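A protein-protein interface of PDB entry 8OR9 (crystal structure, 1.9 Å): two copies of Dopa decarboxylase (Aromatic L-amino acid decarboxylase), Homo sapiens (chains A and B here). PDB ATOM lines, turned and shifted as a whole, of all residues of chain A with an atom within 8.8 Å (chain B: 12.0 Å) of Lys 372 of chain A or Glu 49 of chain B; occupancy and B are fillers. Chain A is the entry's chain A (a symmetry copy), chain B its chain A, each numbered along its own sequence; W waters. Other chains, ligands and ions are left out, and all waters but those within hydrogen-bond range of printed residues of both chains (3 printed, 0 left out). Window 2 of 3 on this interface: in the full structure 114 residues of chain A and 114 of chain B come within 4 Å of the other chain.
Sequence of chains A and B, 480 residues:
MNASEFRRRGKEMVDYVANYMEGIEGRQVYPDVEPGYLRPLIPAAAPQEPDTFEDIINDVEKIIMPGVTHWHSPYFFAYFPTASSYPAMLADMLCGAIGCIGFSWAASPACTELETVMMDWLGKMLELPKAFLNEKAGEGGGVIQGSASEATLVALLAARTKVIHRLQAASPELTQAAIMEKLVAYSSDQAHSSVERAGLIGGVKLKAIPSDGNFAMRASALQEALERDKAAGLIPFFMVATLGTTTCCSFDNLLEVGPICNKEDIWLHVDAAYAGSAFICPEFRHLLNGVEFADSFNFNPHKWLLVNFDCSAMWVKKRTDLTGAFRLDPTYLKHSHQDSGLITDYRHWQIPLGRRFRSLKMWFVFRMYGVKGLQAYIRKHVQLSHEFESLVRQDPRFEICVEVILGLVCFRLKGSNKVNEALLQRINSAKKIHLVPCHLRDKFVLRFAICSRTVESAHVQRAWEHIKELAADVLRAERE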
ATOM      1  N   MET A 125      -2.567 -11.485 -34.247  1.00  0.00           N
ATOM      2  CA  MET A 125      -3.178 -10.997 -33.013  1.00  0.00           C
ATOM      3  C   MET A 125      -2.659  -9.616 -32.636  1.00  0.00           C
ATOM      4  O   MET A 125      -3.401  -8.807 -32.069  1.00  0.00           O
ATOM      5  CB  MET A 125      -2.927 -11.986 -31.875  1.00  0.00           C
ATOM      6  CG  MET A 125      -3.683 -13.297 -32.020  1.00  0.00           C
ATOM      7  SD  MET A 125      -3.066 -14.580 -30.911  1.00  0.00           S
ATOM      8  CE  MET A 125      -3.384 -13.818 -29.321  1.00  0.00           C
ATOM      9  N   ILE A 280      -2.058  -6.976 -28.309  1.00  0.00           N
ATOM     10  CA  ILE A 280      -3.200  -7.718 -28.829  1.00  0.00           C
ATOM     11  C   ILE A 280      -4.523  -7.056 -28.483  1.00  0.00           C
ATOM     12  O   ILE A 280      -5.562  -7.435 -29.039  1.00  0.00           O
ATOM     13  CB  ILE A 280      -3.217  -9.172 -28.311  1.00  0.00           C
ATOM     14  CG1 ILE A 280      -3.558  -9.205 -26.819  1.00  0.00           C
ATOM     15  CG2 ILE A 280      -1.887  -9.852 -28.589  1.00  0.00           C
ATOM     16  CD1 ILE A 280      -3.812 -10.602 -26.275  1.00  0.00           C
ATOM     17  N   CYS A 281      -4.514  -6.081 -27.562  1.00  0.00           N
ATOM     18  CA  CYS A 281      -5.687  -5.284 -27.221  1.00  0.00           C
ATOM     19  C   CYS A 281      -5.704  -4.015 -28.065  1.00  0.00           C
ATOM     20  O   CYS A 281      -4.708  -3.283 -28.088  1.00  0.00           O
ATOM     21  CB  CYS A 281      -5.689  -4.918 -25.743  1.00  0.00           C
ATOM     22  SG  CYS A 281      -5.682  -6.320 -24.604  1.00  0.00           S
ATOM     23  N   VAL A 365      -1.957 -22.662 -25.378  1.00  0.00           N
ATOM     24  CA  VAL A 365      -2.397 -21.456 -24.678  1.00  0.00           C
ATOM     25  C   VAL A 365      -3.375 -20.664 -25.539  1.00  0.00           C
ATOM     26  O   VAL A 365      -4.432 -20.230 -25.065  1.00  0.00           O
ATOM     27  CB  VAL A 365      -1.188 -20.599 -24.263  1.00  0.00           C
ATOM     28  CG1 VAL A 365      -1.641 -19.196 -23.875  1.00  0.00           C
ATOM     29  CG2 VAL A 365      -0.443 -21.254 -23.113  1.00  0.00           C
ATOM     30  N   PHE A 366      -3.036 -20.461 -26.815  1.00  0.00           N
ATOM     31  CA  PHE A 366      -3.905 -19.687 -27.697  1.00  0.00           C
ATOM     32  C   PHE A 366      -5.266 -20.353 -27.858  1.00  0.00           C
ATOM     33  O   PHE A 366      -6.293 -19.672 -27.947  1.00  0.00           O
ATOM     34  CB  PHE A 366      -3.247 -19.494 -29.065  1.00  0.00           C
ATOM     35  CG  PHE A 366      -1.980 -18.679 -29.033  1.00  0.00           C
ATOM     36  CD1 PHE A 366      -1.681 -17.861 -27.954  1.00  0.00           C
ATOM     37  CD2 PHE A 366      -1.085 -18.736 -30.090  1.00  0.00           C
ATOM     38  CE1 PHE A 366      -0.516 -17.116 -27.933  1.00  0.00           C
ATOM     39  CE2 PHE A 366       0.081 -17.993 -30.075  1.00  0.00           C
ATOM     40  CZ  PHE A 366       0.367 -17.183 -28.997  1.00  0.00           C
ATOM     41  N   ARG A 367      -5.294 -21.688 -27.890  1.00  0.00           N
ATOM     42  CA  ARG A 367      -6.542 -22.398 -28.148  1.00  0.00           C
ATOM     43  C   ARG A 367      -7.395 -22.531 -26.891  1.00  0.00           C
ATOM     44  O   ARG A 367      -8.620 -22.384 -26.957  1.00  0.00           O
ATOM     45  CB  ARG A 367      -6.251 -23.777 -28.745  1.00  0.00           C
ATOM     46  CG  ARG A 367      -5.730 -23.740 -30.179  1.00  0.00           C
ATOM     47  CD  ARG A 367      -5.628 -25.141 -30.779  1.00  0.00           C
ATOM     48  NE  ARG A 367      -6.941 -25.720 -31.056  1.00  0.00           N
ATOM     49  CZ  ARG A 367      -7.135 -26.926 -31.581  1.00  0.00           C
ATOM     50  NH1 ARG A 367      -6.100 -27.698 -31.888  1.00  0.00           N
ATOM     51  NH2 ARG A 367      -8.369 -27.365 -31.797  1.00  0.00           N
ATOM     52  N   MET A 368      -6.775 -22.807 -25.741  1.00  0.00           N
ATOM     53  CA  MET A 368      -7.540 -23.011 -24.517  1.00  0.00           C
ATOM     54  C   MET A 368      -8.001 -21.705 -23.882  1.00  0.00           C
ATOM     55  O   MET A 368      -8.986 -21.712 -23.134  1.00  0.00           O
ATOM     56  CB  MET A 368      -6.722 -23.820 -23.508  1.00  0.00           C
ATOM     57  CG  MET A 368      -6.332 -25.196 -24.023  1.00  0.00           C
ATOM     58  SD  MET A 368      -5.942 -26.405 -22.749  1.00  0.00           S
ATOM     59  CE  MET A 368      -7.580 -26.760 -22.111  1.00  0.00           C
ATOM     60  N   TYR A 369      -7.320 -20.594 -24.155  1.00  0.00           N
ATOM     61  CA  TYR A 369      -7.774 -19.296 -23.673  1.00  0.00           C
ATOM     62  C   TYR A 369      -8.591 -18.553 -24.719  1.00  0.00           C
ATOM     63  O   TYR A 369      -9.576 -17.889 -24.380  1.00  0.00           O
ATOM     64  CB  TYR A 369      -6.582 -18.434 -23.252  1.00  0.00           C
ATOM     65  CG  TYR A 369      -6.118 -18.675 -21.835  1.00  0.00           C
ATOM     66  CD1 TYR A 369      -6.724 -18.023 -20.768  1.00  0.00           C
ATOM     67  CD2 TYR A 369      -5.075 -19.549 -21.563  1.00  0.00           C
ATOM     68  CE1 TYR A 369      -6.305 -18.239 -19.468  1.00  0.00           C
ATOM     69  CE2 TYR A 369      -4.649 -19.773 -20.268  1.00  0.00           C
ATOM     70  CZ  TYR A 369      -5.268 -19.114 -19.223  1.00  0.00           C
ATOM     71  OH  TYR A 369      -4.851 -19.330 -17.929  1.00  0.00           O
ATOM     72  N   GLY A 370      -8.206 -18.659 -25.984  1.00  0.00           N
ATOM     73  CA  GLY A 370      -8.767 -17.818 -27.017  1.00  0.00           C
ATOM     74  C   GLY A 370      -8.204 -16.409 -26.954  1.00  0.00           C
ATOM     75  O   GLY A 370      -7.646 -15.971 -25.948  1.00  0.00           O
ATOM     76  N   VAL A 371      -8.345 -15.691 -28.069  1.00  0.00           N
ATOM     77  CA  VAL A 371      -7.858 -14.314 -28.117  1.00  0.00           C
ATOM     78  C   VAL A 371      -8.561 -13.465 -27.063  1.00  0.00           C
ATOM     79  O   VAL A 371      -7.936 -12.629 -26.398  1.00  0.00           O
ATOM     80  CB  VAL A 371      -8.037 -13.734 -29.532  1.00  0.00           C
ATOM     81  CG1 VAL A 371      -7.678 -12.257 -29.551  1.00  0.00           C
ATOM     82  CG2 VAL A 371      -7.182 -14.502 -30.529  1.00  0.00           C
ATOM     83  N   LYS A 372      -9.864 -13.685 -26.874  1.00  0.00           N
ATOM     84  CA  LYS A 372     -10.609 -12.904 -25.893  1.00  0.00           C
ATOM     85  C   LYS A 372     -10.203 -13.246 -24.465  1.00  0.00           C
ATOM     86  O   LYS A 372     -10.214 -12.369 -23.595  1.00  0.00           O
ATOM     87  CB  LYS A 372     -12.109 -13.119 -26.089  1.00  0.00           C
ATOM     88  CG  LYS A 372     -12.617 -12.600 -27.422  1.00  0.00           C
ATOM     89  CD  LYS A 372     -14.116 -12.776 -27.558  1.00  0.00           C
ATOM     90  CE  LYS A 372     -14.605 -12.224 -28.886  1.00  0.00           C
ATOM     91  NZ  LYS A 372     -16.087 -12.117 -28.934  1.00  0.00           N
ATOM     92  N   GLY A 373      -9.848 -14.505 -24.202  1.00  0.00           N
ATOM     93  CA  GLY A 373      -9.361 -14.858 -22.879  1.00  0.00           C
ATOM     94  C   GLY A 373      -8.034 -14.195 -22.558  1.00  0.00           C
ATOM     95  O   GLY A 373      -7.804 -13.760 -21.425  1.00  0.00           O
ATOM     96  N   LEU A 374      -7.144 -14.109 -23.548  1.00  0.00           N
ATOM     97  CA  LEU A 374      -5.872 -13.426 -23.338  1.00  0.00           C
ATOM     98  C   LEU A 374      -6.074 -11.923 -23.189  1.00  0.00           C
ATOM     99  O   LEU A 374      -5.404 -11.280 -22.373  1.00  0.00           O
ATOM    100  CB  LEU A 374      -4.915 -13.730 -24.491  1.00  0.00           C
ATOM    101  CG  LEU A 374      -4.488 -15.193 -24.641  1.00  0.00           C
ATOM    102  CD1 LEU A 374      -3.625 -15.374 -25.881  1.00  0.00           C
ATOM    103  CD2 LEU A 374      -3.756 -15.676 -23.397  1.00  0.00           C
ATOM    104  N   GLN A 375      -6.990 -11.346 -23.970  1.00  0.00           N
ATOM    105  CA  GLN A 375      -7.264  -9.917 -23.847  1.00  0.00           C
ATOM    106  C   GLN A 375      -7.808  -9.581 -22.464  1.00  0.00           C
ATOM    107  O   GLN A 375      -7.430  -8.565 -21.869  1.00  0.00           O
ATOM    108  CB  GLN A 375      -8.247  -9.472 -24.931  1.00  0.00           C
ATOM    109  CG  GLN A 375      -7.643  -9.365 -26.319  1.00  0.00           C
ATOM    110  CD  GLN A 375      -8.689  -9.084 -27.380  1.00  0.00           C
ATOM    111  OE1 GLN A 375      -9.813  -9.586 -27.309  1.00  0.00           O
ATOM    112  NE2 GLN A 375      -8.327  -8.274 -28.369  1.00  0.00           N
ATOM    113  N   ALA A 376      -8.693 -10.429 -21.934  1.00  0.00           N
ATOM    114  CA  ALA A 376      -9.227 -10.203 -20.596  1.00  0.00           C
ATOM    115  C   ALA A 376      -8.130 -10.297 -19.542  1.00  0.00           C
ATOM    116  O   ALA A 376      -8.146  -9.557 -18.552  1.00  0.00           O
ATOM    117  CB  ALA A 376     -10.343 -11.204 -20.303  1.00  0.00           C
ATOM    118  N   TYR A 377      -7.167 -11.200 -19.743  1.00  0.00           N
ATOM    119  CA  TYR A 377      -6.056 -11.333 -18.804  1.00  0.00           C
ATOM    120  C   TYR A 377      -5.190 -10.080 -18.792  1.00  0.00           C
ATOM    121  O   TYR A 377      -4.781  -9.608 -17.725  1.00  0.00           O
ATOM    122  CB  TYR A 377      -5.232 -12.573 -19.162  1.00  0.00           C
ATOM    123  CG  TYR A 377      -3.804 -12.582 -18.659  1.00  0.00           C
ATOM    124  CD1 TYR A 377      -3.500 -13.000 -17.369  1.00  0.00           C
ATOM    125  CD2 TYR A 377      -2.754 -12.197 -19.486  1.00  0.00           C
ATOM    126  CE1 TYR A 377      -2.191 -13.023 -16.912  1.00  0.00           C
ATOM    127  CE2 TYR A 377      -1.447 -12.216 -19.038  1.00  0.00           C
ATOM    128  CZ  TYR A 377      -1.170 -12.626 -17.752  1.00  0.00           C
ATOM    129  OH  TYR A 377       0.135 -12.645 -17.314  1.00  0.00           O
ATOM    130  N   ILE A 378      -4.904  -9.526 -19.973  1.00  0.00           N
ATOM    131  CA  ILE A 378      -4.114  -8.299 -20.059  1.00  0.00           C
ATOM    132  C   ILE A 378      -4.852  -7.144 -19.395  1.00  0.00           C
ATOM    133  O   ILE A 378      -4.280  -6.390 -18.598  1.00  0.00           O
ATOM    134  CB  ILE A 378      -3.787  -7.976 -21.529  1.00  0.00           C
ATOM    135  CG1 ILE A 378      -2.883  -9.053 -22.136  1.00  0.00           C
ATOM    136  CG2 ILE A 378      -3.162  -6.589 -21.645  1.00  0.00           C
ATOM    137  CD1 ILE A 378      -1.487  -9.080 -21.562  1.00  0.00           C
ATOM    138  N   ARG A 379      -6.138  -6.986 -19.719  1.00  0.00           N
ATOM    139  CA  ARG A 379      -6.888  -5.832 -19.236  1.00  0.00           C
ATOM    140  C   ARG A 379      -7.092  -5.878 -17.728  1.00  0.00           C
ATOM    141  O   ARG A 379      -7.127  -4.825 -17.080  1.00  0.00           O
ATOM    142  CB  ARG A 379      -8.231  -5.742 -19.962  1.00  0.00           C
ATOM    143  CG  ARG A 379      -8.095  -5.289 -21.407  1.00  0.00           C
ATOM    144  CD  ARG A 379      -9.325  -5.622 -22.232  1.00  0.00           C
ATOM    145  NE  ARG A 379      -9.213  -5.072 -23.579  1.00  0.00           N
ATOM    146  CZ  ARG A 379      -9.904  -5.503 -24.628  1.00  0.00           C
ATOM    147  NH1 ARG A 379     -10.767  -6.503 -24.492  1.00  0.00           N
ATOM    148  NH2 ARG A 379      -9.731  -4.934 -25.814  1.00  0.00           N
ATOM    149  N   MET B   1      -8.186 -21.646 -17.212  1.00  0.00           N
ATOM    150  CA  MET B   1      -8.044 -22.951 -16.578  1.00  0.00           C
ATOM    151  C   MET B   1      -7.538 -22.800 -15.146  1.00  0.00           C
ATOM    152  O   MET B   1      -6.536 -22.126 -14.909  1.00  0.00           O
ATOM    153  CB  MET B   1      -7.094 -23.833 -17.391  1.00  0.00           C
ATOM    154  CG  MET B   1      -7.111 -25.301 -17.015  1.00  0.00           C
ATOM    155  SD  MET B   1      -6.341 -26.307 -18.296  1.00  0.00           S
ATOM    156  CE  MET B   1      -6.195 -27.867 -17.451  1.00  0.00           C
ATOM    157  N   PRO B  43      -6.509 -23.736 -38.731  1.00  0.00           N
ATOM    158  CA  PRO B  43      -7.003 -22.422 -39.161  1.00  0.00           C
ATOM    159  C   PRO B  43      -5.889 -21.397 -39.319  1.00  0.00           C
ATOM    160  O   PRO B  43      -4.794 -21.527 -38.767  1.00  0.00           O
ATOM    161  CB  PRO B  43      -7.967 -22.021 -38.038  1.00  0.00           C
ATOM    162  CG  PRO B  43      -8.418 -23.316 -37.458  1.00  0.00           C
ATOM    163  CD  PRO B  43      -7.220 -24.223 -37.535  1.00  0.00           C
ATOM    164  N   ALA B  45      -6.031 -18.304 -38.265  1.00  0.00           N
ATOM    165  CA  ALA B  45      -6.009 -17.354 -37.163  1.00  0.00           C
ATOM    166  C   ALA B  45      -6.370 -18.068 -35.869  1.00  0.00           C
ATOM    167  O   ALA B  45      -7.053 -19.095 -35.871  1.00  0.00           O
ATOM    168  CB  ALA B  45      -6.971 -16.182 -37.409  1.00  0.00           C
ATOM    169  N   ALA B  46      -5.898 -17.506 -34.759  1.00  0.00           N
ATOM    170  CA  ALA B  46      -6.210 -18.057 -33.451  1.00  0.00           C
ATOM    171  C   ALA B  46      -7.710 -17.963 -33.174  1.00  0.00           C
ATOM    172  O   ALA B  46      -8.387 -17.056 -33.669  1.00  0.00           O
ATOM    173  CB  ALA B  46      -5.431 -17.318 -32.365  1.00  0.00           C
ATOM    174  N   PRO B  47      -8.258 -18.892 -32.392  1.00  0.00           N
ATOM    175  CA  PRO B  47      -9.688 -18.829 -32.079  1.00  0.00           C
ATOM    176  C   PRO B  47      -9.987 -17.685 -31.122  1.00  0.00           C
ATOM    177  O   PRO B  47      -9.216 -17.405 -30.200  1.00  0.00           O
ATOM    178  CB  PRO B  47      -9.968 -20.190 -31.434  1.00  0.00           C
ATOM    179  CG  PRO B  47      -8.661 -20.567 -30.812  1.00  0.00           C
ATOM    180  CD  PRO B  47      -7.601 -20.044 -31.749  1.00  0.00           C
ATOM    181  N   GLN B  48     -11.113 -17.011 -31.358  1.00  0.00           N
ATOM    182  CA  GLN B  48     -11.526 -15.927 -30.472  1.00  0.00           C
ATOM    183  C   GLN B  48     -12.062 -16.475 -29.155  1.00  0.00           C
ATOM    184  O   GLN B  48     -11.722 -15.975 -28.076  1.00  0.00           O
ATOM    185  CB  GLN B  48     -12.571 -15.054 -31.168  1.00  0.00           C
ATOM    186  CG  GLN B  48     -12.003 -14.194 -32.290  1.00  0.00           C
ATOM    187  CD  GLN B  48     -11.179 -13.028 -31.775  1.00  0.00           C
ATOM    188  OE1 GLN B  48     -11.575 -12.346 -30.830  1.00  0.00           O
ATOM    189  NE2 GLN B  48     -10.026 -12.794 -32.391  1.00  0.00           N
ATOM    190  N   GLU B  49     -12.913 -17.493 -29.228  1.00  0.00           N
ATOM    191  CA  GLU B  49     -13.389 -18.256 -28.086  1.00  0.00           C
ATOM    192  C   GLU B  49     -12.588 -19.541 -27.945  1.00  0.00           C
ATOM    193  O   GLU B  49     -12.043 -20.053 -28.925  1.00  0.00           O
ATOM    194  CB  GLU B  49     -14.880 -18.579 -28.243  1.00  0.00           C
ATOM    195  CG  GLU B  49     -15.759 -17.369 -28.538  1.00  0.00           C
ATOM    196  CD  GLU B  49     -15.970 -16.479 -27.326  1.00  0.00           C
ATOM    197  OE1 GLU B  49     -15.687 -16.926 -26.195  1.00  0.00           O
ATOM    198  OE2 GLU B  49     -16.430 -15.334 -27.505  1.00  0.00           O
ATOM    199  N   PRO B  50     -12.491 -20.095 -26.739  1.00  0.00           N
ATOM    200  CA  PRO B  50     -11.587 -21.230 -26.527  1.00  0.00           C
ATOM    201  C   PRO B  50     -12.066 -22.506 -27.201  1.00  0.00           C
ATOM    202  O   PRO B  50     -13.265 -22.744 -27.367  1.00  0.00           O
ATOM    203  CB  PRO B  50     -11.572 -21.396 -25.001  1.00  0.00           C
ATOM    204  CG  PRO B  50     -12.175 -20.142 -24.451  1.00  0.00           C
ATOM    205  CD  PRO B  50     -13.137 -19.670 -25.488  1.00  0.00           C
ATOM    206  N   ASP B  51     -11.096 -23.330 -27.591  1.00  0.00           N
ATOM    207  CA  ASP B  51     -11.334 -24.703 -28.010  1.00  0.00           C
ATOM    208  C   ASP B  51     -11.328 -25.623 -26.791  1.00  0.00           C
ATOM    209  O   ASP B  51     -10.886 -25.252 -25.701  1.00  0.00           O
ATOM    210  CB  ASP B  51     -10.275 -25.158 -29.018  1.00  0.00           C
ATOM    211  CG  ASP B  51     -10.369 -24.428 -30.346  1.00  0.00           C
ATOM    212  OD1 ASP B  51     -11.479 -23.990 -30.713  1.00  0.00           O
ATOM    213  OD2 ASP B  51      -9.329 -24.300 -31.030  1.00  0.00           O
ATOM    214  N   THR B  52     -11.819 -26.843 -26.985  1.00  0.00           N
ATOM    215  CA  THR B  52     -11.836 -27.838 -25.922  1.00  0.00           C
ATOM    216  C   THR B  52     -10.535 -28.631 -25.906  1.00  0.00           C
ATOM    217  O   THR B  52      -9.847 -28.757 -26.924  1.00  0.00           O
ATOM    218  CB  THR B  52     -13.018 -28.797 -26.085  1.00  0.00           C
ATOM    219  OG1 THR B  52     -12.843 -29.577 -27.276  1.00  0.00           O
ATOM    220  CG2 THR B  52     -14.329 -28.026 -26.175  1.00  0.00           C
ATOM    221  N   PHE B  53     -10.200 -29.162 -24.726  1.00  0.00           N
ATOM    222  CA  PHE B  53      -9.043 -30.043 -24.597  1.00  0.00           C
ATOM    223  C   PHE B  53      -9.201 -31.285 -25.465  1.00  0.00           C
ATOM    224  O   PHE B  53      -8.223 -31.786 -26.032  1.00  0.00           O
ATOM    225  CB  PHE B  53      -8.853 -30.427 -23.126  1.00  0.00           C
ATOM    226  CG  PHE B  53      -7.643 -31.283 -22.859  1.00  0.00           C
ATOM    227  CD1 PHE B  53      -6.371 -30.734 -22.864  1.00  0.00           C
ATOM    228  CD2 PHE B  53      -7.782 -32.633 -22.573  1.00  0.00           C
ATOM    229  CE1 PHE B  53      -5.258 -31.519 -22.611  1.00  0.00           C
ATOM    230  CE2 PHE B  53      -6.675 -33.421 -22.313  1.00  0.00           C
ATOM    231  CZ  PHE B  53      -5.412 -32.862 -22.326  1.00  0.00           C
ATOM    232  N   ASP B  55     -10.749 -31.461 -28.364  1.00  0.00           N
ATOM    233  CA  ASP B  55     -10.430 -31.058 -29.730  1.00  0.00           C
ATOM    234  C   ASP B  55      -8.923 -30.954 -29.935  1.00  0.00           C
ATOM    235  O   ASP B  55      -8.404 -31.342 -30.988  1.00  0.00           O
ATOM    236  CB  ASP B  55     -11.112 -29.725 -30.046  1.00  0.00           C
ATOM    237  CG  ASP B  55     -10.939 -29.298 -31.494  1.00  0.00           C
ATOM    238  OD1 ASP B  55     -10.640 -30.159 -32.349  1.00  0.00           O
ATOM    239  OD2 ASP B  55     -11.106 -28.091 -31.777  1.00  0.00           O
ATOM    240  N   ILE B  56      -8.204 -30.447 -28.933  1.00  0.00           N
ATOM    241  CA  ILE B  56      -6.767 -30.230 -29.085  1.00  0.00           C
ATOM    242  C   ILE B  56      -6.022 -31.559 -29.110  1.00  0.00           C
ATOM    243  O   ILE B  56      -5.148 -31.783 -29.955  1.00  0.00           O
ATOM    244  CB  ILE B  56      -6.248 -29.309 -27.967  1.00  0.00           C
ATOM    245  CG1 ILE B  56      -6.789 -27.895 -28.168  1.00  0.00           C
ATOM    246  CG2 ILE B  56      -4.727 -29.307 -27.939  1.00  0.00           C
ATOM    247  CD1 ILE B  56      -6.753 -27.050 -26.925  1.00  0.00           C
ATOM    248  N   ASP B  59      -6.396 -33.243 -32.318  1.00  0.00           N
ATOM    249  CA  ASP B  59      -5.521 -32.657 -33.330  1.00  0.00           C
ATOM    250  C   ASP B  59      -4.077 -33.116 -33.166  1.00  0.00           C
ATOM    251  O   ASP B  59      -3.348 -33.223 -34.159  1.00  0.00           O
ATOM    252  CB  ASP B  59      -5.595 -31.132 -33.279  1.00  0.00           C
ATOM    253  CG  ASP B  59      -6.844 -30.583 -33.944  1.00  0.00           C
ATOM    254  OD1 ASP B  59      -7.487 -31.328 -34.713  1.00  0.00           O
ATOM    255  OD2 ASP B  59      -7.176 -29.403 -33.703  1.00  0.00           O
HETATM  256  O   HOH W   1      -4.199 -21.481 -16.456  1.00  0.00           O
HETATM  257  O   HOH W   2     -11.128  -9.936 -29.639  1.00  0.00           O
HETATM  258  O   HOH W   3      -7.832 -23.573 -33.504  1.00  0.00           O
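The backbone NH (N) of Lys 372 of chain A lies within hydrogen-bond range of the backbone carbonyl oxygen (O) of Gln 48 of chain B (3.2 Å). The side-chain carboxylate of Asp 59 of chain B lies within salt-bridge range of the guanidinium group of Arg 367 of chain A. OD2 of Asp 51 of chain B is in salt-bridge range of NE of Arg 367 of chain A, 2.8 Å away. The side-chain carboxylate (OE2) of Glu 49 of chain B lies within salt-bridge range of the side-chain amino group (NZ) of Lys 372 of chain A (3.5 Å). The side-chain carboxylate (OD2) of Asp 55 of chain B lies within salt-bridge range of the guanidinium group (NH2) of Arg 367 of chain A, at 2.8 Å. O of Pro 47 of chain B is in hydrogen-bond range of N of Val 371 of chain A (2.9 Å). The backbone carbonyl oxygen (O) of Gln 48 of chain B lies within hydrogen-bond range of the backbone NH (N) of Val 371 of chain A (3.4 Å).
N of Asp 55 of chain B is in hydrogen-bond range of OG1 of Thr 52 of chain B (3.0 Å).
CB of Ala 46 of chain B touches SD of Met 125 of chain A (3.9 Å). O of Phe 366 of chain A touches CG of Pro 47 of chain B, at 3.8 Å. Pro 47 of chain B touches Arg 367 of chain A. Pro 50 of chain B touches Arg 367 of chain A (CA to O, 3.2 Å). CZ of Arg 367 of chain A touches CG1 of Ile 56 of chain B, at 3.6 Å. O of Met 368 of chain A touches CB of Pro 50 of chain B, at 3.2 Å. CD1 of Ile 56 of chain B touches CG of Met 368 of chain A (3.5 Å). Tyr 369 of chain A touches Pro 50 of chain B (O to CG, 3.4 Å). Gln 48 of chain B touches Gly 370 of chain A (O to CA, 3.6 Å). Ala 46 of chain B touches Val 371 of chain A.
Of chain B, only Gln 48 (3.2 Å) and Glu 49 (3.4 Å) come within 4 Å of Lys 372 of chain A. Glu 49 of chain B touches one residue of chain A. Val 371 of chain A touches just these residues of chain B: Ala 46 (3.8 Å), Pro 47 (2.9 Å) and Gln 48 (3.4 Å). No residue of chain B comes within 4 Å of Gln 375 of chain A. No residue of chain B comes within 4 Å of Ala 376 of chain A. Pro 50 of chain B touches three residues of chain A. Printed residues of chain A within 4 Å of Pro 47 of chain B: Phe 366, Arg 367, Gly 370 and Val 371. Printed residues of chain B within 4 Å of Arg 367 of chain A: Pro 47 (3.9 Å), Pro 50 (3.2 Å), Asp 51 (2.7 Å), Asp 55 (2.8 Å), Ile 56 (3.6 Å) and Asp 59 (2.7 Å). Printed residues of chain A within 4 Å of Asp 59 of chain B: Arg 367. Printed residues of chain B within 4 Å of Met 125 of chain A: Ala 46. Arg 379 of chain A touches none of the printed residues of chain B. Phe 53 of chain B touches none of the printed residues of chain A.
Of the 14 printed residues of chain B, 9 touch a printed residue of chain A. Hydrophobic or aromatic side chains of chain B that line the printed part of chain A: Ala 46, Pro 47, Pro 50 and Ile 56. Of the 18 printed residues of chain A, 8 touch a printed residue of chain B. Hydrophobic or aromatic side chains of chain A within 4 Å of the printed part of chain B: Met 125, Met 368 and Val 371. Among the printed residues, 18 pairs touch across the chains.
No position is printed for both chains. Of the 18 pairs that touch across the chains among the printed residues, none has its exchanged pair printed and touching as well.
Water W1 bridges OH of Tyr 369 of chain A (2.7 Å) and O of Met 1 of chain B (2.9 Å). Water W2 bridges OE1 of Gln 375 of chain A (2.7 Å) and OE1 of Gln 48 of chain B (2.7 Å). Water W3 bridges OD2 of Asp 51 of chain B and NE of Arg 367 of chain A.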
